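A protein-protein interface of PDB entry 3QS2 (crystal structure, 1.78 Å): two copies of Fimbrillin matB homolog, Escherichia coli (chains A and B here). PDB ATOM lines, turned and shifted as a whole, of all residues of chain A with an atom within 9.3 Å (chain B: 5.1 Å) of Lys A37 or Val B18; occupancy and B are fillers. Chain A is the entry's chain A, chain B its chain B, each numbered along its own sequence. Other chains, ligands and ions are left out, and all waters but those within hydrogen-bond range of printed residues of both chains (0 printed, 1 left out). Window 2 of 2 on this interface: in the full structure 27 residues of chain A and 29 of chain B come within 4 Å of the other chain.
The backbone carbonyl oxygen (O) of Val B18 is in hydrogen-bond range of the backbone NH (N) of Trp B186 (2.7 Å).
The backbone NH (N) of Ala B184 lies within hydrogen-bond range of the backbone carbonyl oxygen (O) of Ala B20, 2.9 Å away.
Of the 12 printed residues of chain B, 7 touch a printed residue of chain A.
Printed residues of chain B that touch a printed residue of chain A: Val B18, Thr B19, Ala B20, Ala B67, Ile B68, Glu B69 and Trp B186.
Hydrophobic or aromatic side chains of chain B that line the printed part of chain A: Val B18, Ala B20, Ile B68 and Trp B186.
Hydrophobic or aromatic side chains of chain A within 4 Å of the printed part of chain B: Leu A38.
Along chain A the printed residues that touch a printed residue of chain B span positions 36 to 39.
Among the printed residues, 12 pairs touch across the chains.
Among the printed residues, no Asp or Glu carboxylate lies within 4 Å of a Lys or Arg side-chain nitrogen of the other chain.
Lys A37 touches seven residues of chain B.
Of chain A, only Lys A37 comes within 4 Å of Val B18.
Asp B17 touches none of the printed residues of chain A.
Of the printed residues of chain A, Trp B186 touches Lys A37 (3.4 Å).
Of the printed residues of chain B, Leu A38 touches Ala B20, Ala B67 and Ile B68.
Of the printed residues of chain A, Ile B68 touches Lys A37 and Leu A38.
Of the printed residues of chain A, Ala B20 touches Lys A37 (3.7 Å) and Leu A38 (3.8 Å).
Printed residues of chain B within 4 Å of Ser A36: Glu B69 (3.1 Å).
Thr A35 touches none of the printed residues of chain B.
The nearest printed residue of chain B that does not touch Lys A37 is Ala B184 (5.9 Å).
The nearest residue of chain A that does not touch Val B18 is Leu A38 (8.4 Å).
No position is printed for both chains.
Of the 12 pairs that touch across the chains among the printed residues, none has its exchanged pair printed and touching as well.
Among the printed residues, merely in contact across the chains: Lys A37 with Ile B68 (3.2 Å), Lys A37 with Thr B19 (3.3 Å), Lys A37 with Trp B186 (3.4 Å), Leu A38 with Ala B67 (3.5 Å), Lys A37 with Ala B20 (3.7 Å), Lys A37 with Val B18 (3.7 Å), Leu A38 with Ala B20 (3.8 Å), Lys A37 with Ala B67 (3.9 Å) and Leu A38 with Ile B68 (3.9 Å).
The side-chain carboxylate (OE1) of Glu B69 sits close to the backbone carbonyl oxygen (O) of Ser A36 (3.1 Å).
O of Val A39 lies within hydrogen-bond range of N of Ala B67.
The backbone carbonyl oxygen (O) of Lys A37 is in hydrogen-bond range of the backbone NH (N) of Glu B69 (3.1 Å).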
ATOM      1  N   THR A  34     -13.325  -3.480  -1.562  1.00  0.00           N
ATOM      2  CA  THR A  34     -13.065  -4.872  -1.804  1.00  0.00           C
ATOM      3  C   THR A  34     -14.316  -5.528  -2.391  1.00  0.00           C
ATOM      4  O   THR A  34     -15.410  -5.038  -2.269  1.00  0.00           O
ATOM      5  CB  THR A  34     -12.687  -5.671  -0.555  1.00  0.00           C
ATOM      6  OG1 THR A  34     -13.658  -5.501   0.449  1.00  0.00           O
ATOM      7  CG2 THR A  34     -11.329  -5.341  -0.026  1.00  0.00           C
ATOM      8  N   THR A  35     -14.112  -6.642  -3.044  1.00  0.00           N
ATOM      9  CA  THR A  35     -15.182  -7.508  -3.482  1.00  0.00           C
ATOM     10  C   THR A  35     -16.180  -7.772  -2.381  1.00  0.00           C
ATOM     11  O   THR A  35     -15.790  -7.939  -1.259  1.00  0.00           O
ATOM     12  CB  THR A  35     -14.595  -8.842  -3.772  1.00  0.00           C
ATOM     13  N   SER A  36     -17.447  -7.824  -2.716  1.00  0.00           N
ATOM     14  CA  SER A  36     -18.453  -8.236  -1.770  1.00  0.00           C
ATOM     15  C   SER A  36     -19.236  -9.448  -2.264  1.00  0.00           C
ATOM     16  O   SER A  36     -20.342  -9.642  -1.934  1.00  0.00           O
ATOM     17  CB  SER A  36     -19.370  -7.072  -1.387  1.00  0.00           C
ATOM     18  OG  SER A  36     -19.805  -6.407  -2.521  1.00  0.00           O
ATOM     19  N   LYS A  37     -18.588 -10.276  -3.046  1.00  0.00           N
ATOM     20  CA  LYS A  37     -19.185 -11.536  -3.495  1.00  0.00           C
ATOM     21  C   LYS A  37     -19.502 -12.451  -2.313  1.00  0.00           C
ATOM     22  O   LYS A  37     -20.470 -13.203  -2.356  1.00  0.00           O
ATOM     23  CB  LYS A  37     -18.277 -12.281  -4.466  1.00  0.00           C
ATOM     24  CG  LYS A  37     -18.127 -11.607  -5.825  1.00  0.00           C
ATOM     25  CD  LYS A  37     -17.272 -12.433  -6.775  1.00  0.00           C
ATOM     26  CE  LYS A  37     -15.923 -12.829  -6.146  1.00  0.00           C
ATOM     27  NZ  LYS A  37     -14.969 -11.712  -5.931  1.00  0.00           N
ATOM     28  N   LEU A  38     -18.651 -12.401  -1.292  1.00  0.00           N
ATOM     29  CA  LEU A  38     -18.875 -13.136  -0.037  1.00  0.00           C
ATOM     30  C   LEU A  38     -18.573 -12.248   1.157  1.00  0.00           C
ATOM     31  O   LEU A  38     -17.468 -11.704   1.268  1.00  0.00           O
ATOM     32  CB  LEU A  38     -18.009 -14.397   0.021  1.00  0.00           C
ATOM     33  CG  LEU A  38     -18.004 -15.184   1.347  1.00  0.00           C
ATOM     34  CD1 LEU A  38     -19.348 -15.889   1.556  1.00  0.00           C
ATOM     35  CD2 LEU A  38     -16.875 -16.211   1.372  1.00  0.00           C
ATOM     36  N   VAL A  39     -19.547 -12.095   2.049  1.00  0.00           N
ATOM     37  CA  VAL A  39     -19.357 -11.314   3.267  1.00  0.00           C
ATOM     38  C   VAL A  39     -19.825 -12.175   4.437  1.00  0.00           C
ATOM     39  O   VAL A  39     -20.946 -12.673   4.422  1.00  0.00           O
ATOM     40  CB  VAL A  39     -20.172  -9.983   3.253  1.00  0.00           C
ATOM     41  CG1 VAL A  39     -19.880  -9.173   4.487  1.00  0.00           C
ATOM     42  CG2 VAL A  39     -19.851  -9.166   1.997  1.00  0.00           C
ATOM     43  N   VAL A  40     -18.963 -12.360   5.438  1.00  0.00           N
ATOM     44  CA  VAL A  40     -19.335 -13.167   6.598  1.00  0.00           C
ATOM     45  C   VAL A  40     -19.108 -12.351   7.856  1.00  0.00           C
ATOM     46  O   VAL A  40     -18.007 -11.847   8.077  1.00  0.00           O
ATOM     47  CB  VAL A  40     -18.561 -14.521   6.658  1.00  0.00           C
ATOM     48  CG1 VAL A  40     -18.998 -15.302   7.870  1.00  0.00           C
ATOM     49  CG2 VAL A  40     -18.787 -15.346   5.368  1.00  0.00           C
ATOM     50  N   ALA B  16     -14.275 -20.522 -16.434  1.00  0.00           N
ATOM     51  CA  ALA B  16     -13.530 -20.589 -15.146  1.00  0.00           C
ATOM     52  C   ALA B  16     -14.463 -20.284 -13.976  1.00  0.00           C
ATOM     53  O   ALA B  16     -15.343 -19.419 -14.076  1.00  0.00           O
ATOM     54  CB  ALA B  16     -12.346 -19.620 -15.154  1.00  0.00           C
ATOM     55  N   ASP B  17     -14.281 -20.994 -12.867  1.00  0.00           N
ATOM     56  CA  ASP B  17     -15.116 -20.731 -11.701  1.00  0.00           C
ATOM     57  C   ASP B  17     -14.708 -19.444 -10.988  1.00  0.00           C
ATOM     58  O   ASP B  17     -13.572 -18.984 -11.109  1.00  0.00           O
ATOM     59  CB  ASP B  17     -15.214 -21.945 -10.760  1.00  0.00           C
ATOM     60  CG  ASP B  17     -13.869 -22.557 -10.410  1.00  0.00           C
ATOM     61  OD1 ASP B  17     -12.841 -21.846 -10.438  1.00  0.00           O
ATOM     62  OD2 ASP B  17     -13.851 -23.767 -10.082  1.00  0.00           O
ATOM     63  N   VAL B  18     -15.672 -18.921 -10.225  1.00  0.00           N
ATOM     64  CA  VAL B  18     -15.506 -17.712  -9.442  1.00  0.00           C
ATOM     65  C   VAL B  18     -15.409 -18.112  -7.974  1.00  0.00           C
ATOM     66  O   VAL B  18     -16.125 -19.003  -7.504  1.00  0.00           O
ATOM     67  CB  VAL B  18     -16.642 -16.682  -9.711  1.00  0.00           C
ATOM     68  CG1 VAL B  18     -16.523 -15.488  -8.806  1.00  0.00           C
ATOM     69  CG2 VAL B  18     -16.678 -16.236 -11.163  1.00  0.00           C
ATOM     70  N   THR B  19     -14.413 -17.437  -7.346  1.00  0.00           N
ATOM     71  CA  THR B  19     -14.175 -17.737  -5.947  1.00  0.00           C
ATOM     72  C   THR B  19     -14.138 -16.450  -5.152  1.00  0.00           C
ATOM     73  O   THR B  19     -13.871 -15.373  -5.698  1.00  0.00           O
ATOM     74  CB  THR B  19     -12.833 -18.436  -5.761  1.00  0.00           C
ATOM     75  OG1 THR B  19     -11.811 -17.584  -6.276  1.00  0.00           O
ATOM     76  CG2 THR B  19     -12.794 -19.766  -6.526  1.00  0.00           C
ATOM     77  N   ALA B  20     -14.401 -16.569  -3.860  1.00  0.00           N
ATOM     78  CA  ALA B  20     -14.318 -15.439  -2.956  1.00  0.00           C
ATOM     79  C   ALA B  20     -13.971 -15.982  -1.584  1.00  0.00           C
ATOM     80  O   ALA B  20     -14.203 -17.166  -1.288  1.00  0.00           O
ATOM     81  CB  ALA B  20     -15.628 -14.671  -2.916  1.00  0.00           C
ATOM     82  N   ALA B  67     -23.504 -13.378   3.489  1.00  0.00           N
ATOM     83  CA  ALA B  67     -24.168 -12.711   2.372  1.00  0.00           C
ATOM     84  C   ALA B  67     -23.396 -13.054   1.114  1.00  0.00           C
ATOM     85  O   ALA B  67     -22.175 -12.940   1.101  1.00  0.00           O
ATOM     86  CB  ALA B  67     -24.179 -11.197   2.585  1.00  0.00           C
ATOM     87  N   ILE B  68     -24.096 -13.493   0.071  1.00  0.00           N
ATOM     88  CA  ILE B  68     -23.448 -13.721  -1.215  1.00  0.00           C
ATOM     89  C   ILE B  68     -24.104 -12.901  -2.315  1.00  0.00           C
ATOM     90  O   ILE B  68     -25.292 -12.585  -2.225  1.00  0.00           O
ATOM     91  CB  ILE B  68     -23.413 -15.223  -1.608  1.00  0.00           C
ATOM     92  CG1 ILE B  68     -24.826 -15.808  -1.747  1.00  0.00           C
ATOM     93  CG2 ILE B  68     -22.576 -16.009  -0.580  1.00  0.00           C
ATOM     94  CD1 ILE B  68     -24.837 -17.201  -2.416  1.00  0.00           C
ATOM     95  N   GLU B  69     -23.301 -12.545  -3.316  1.00  0.00           N
ATOM     96  CA  GLU B  69     -23.789 -11.966  -4.566  1.00  0.00           C
ATOM     97  C   GLU B  69     -24.045 -13.082  -5.553  1.00  0.00           C
ATOM     98  O   GLU B  69     -23.182 -13.923  -5.767  1.00  0.00           O
ATOM     99  CB  GLU B  69     -22.735 -11.058  -5.203  1.00  0.00           C
ATOM    100  CG  GLU B  69     -22.300  -9.844  -4.425  1.00  0.00           C
ATOM    101  CD  GLU B  69     -23.409  -9.130  -3.700  1.00  0.00           C
ATOM    102  OE1 GLU B  69     -23.359  -9.109  -2.460  1.00  0.00           O
ATOM    103  OE2 GLU B  69     -24.312  -8.572  -4.359  1.00  0.00           O
ATOM    104  N   ASP B  71     -24.553 -15.231  -9.027  1.00  0.00           N
ATOM    105  CA  ASP B  71     -23.779 -15.437 -10.245  1.00  0.00           C
ATOM    106  C   ASP B  71     -24.703 -16.181 -11.208  1.00  0.00           C
ATOM    107  O   ASP B  71     -24.896 -17.337 -11.055  1.00  0.00           O
ATOM    108  CB  ASP B  71     -22.546 -16.313  -9.990  1.00  0.00           C
ATOM    109  CG  ASP B  71     -21.795 -16.649 -11.243  1.00  0.00           C
ATOM    110  OD1 ASP B  71     -22.304 -16.344 -12.298  1.00  0.00           O
ATOM    111  OD2 ASP B  71     -20.710 -17.187 -11.186  1.00  0.00           O
ATOM    112  N   ALA B 184     -15.926 -19.451  -0.800  1.00  0.00           N
ATOM    113  CA  ALA B 184     -17.059 -19.700  -1.718  1.00  0.00           C
ATOM    114  C   ALA B 184     -16.562 -19.996  -3.129  1.00  0.00           C
ATOM    115  O   ALA B 184     -15.634 -19.359  -3.608  1.00  0.00           O
ATOM    116  CB  ALA B 184     -18.012 -18.496  -1.744  1.00  0.00           C
ATOM    117  N   THR B 185     -17.196 -20.957  -3.796  1.00  0.00           N
ATOM    118  CA  THR B 185     -16.840 -21.250  -5.189  1.00  0.00           C
ATOM    119  C   THR B 185     -18.119 -21.404  -5.991  1.00  0.00           C
ATOM    120  O   THR B 185     -19.015 -22.174  -5.615  1.00  0.00           O
ATOM    121  CB  THR B 185     -16.012 -22.525  -5.304  1.00  0.00           C
ATOM    122  OG1 THR B 185     -14.931 -22.469  -4.375  1.00  0.00           O
ATOM    123  CG2 THR B 185     -15.434 -22.663  -6.711  1.00  0.00           C
ATOM    124  N   TRP B 186     -18.217 -20.633  -7.067  1.00  0.00           N
ATOM    125  CA  TRP B 186     -19.294 -20.790  -8.028  1.00  0.00           C
ATOM    126  C   TRP B 186     -18.696 -21.452  -9.265  1.00  0.00           C
ATOM    127  O   TRP B 186     -17.692 -20.967  -9.809  1.00  0.00           O
ATOM    128  CB  TRP B 186     -19.819 -19.431  -8.455  1.00  0.00           C
ATOM    129  CG  TRP B 186     -20.682 -18.688  -7.479  1.00  0.00           C
ATOM    130  CD1 TRP B 186     -22.043 -18.673  -7.454  1.00  0.00           C
ATOM    131  CD2 TRP B 186     -20.253 -17.805  -6.431  1.00  0.00           C
ATOM    132  NE1 TRP B 186     -22.493 -17.844  -6.465  1.00  0.00           N
ATOM    133  CE2 TRP B 186     -21.416 -17.301  -5.813  1.00  0.00           C
ATOM    134  CE3 TRP B 186     -19.005 -17.399  -5.952  1.00  0.00           C
ATOM    135  CZ2 TRP B 186     -21.369 -16.412  -4.734  1.00  0.00           C
ATOM    136  CZ3 TRP B 186     -18.958 -16.500  -4.878  1.00  0.00           C
ATOM    137  CH2 TRP B 186     -20.136 -16.020  -4.285  1.00  0.00           C
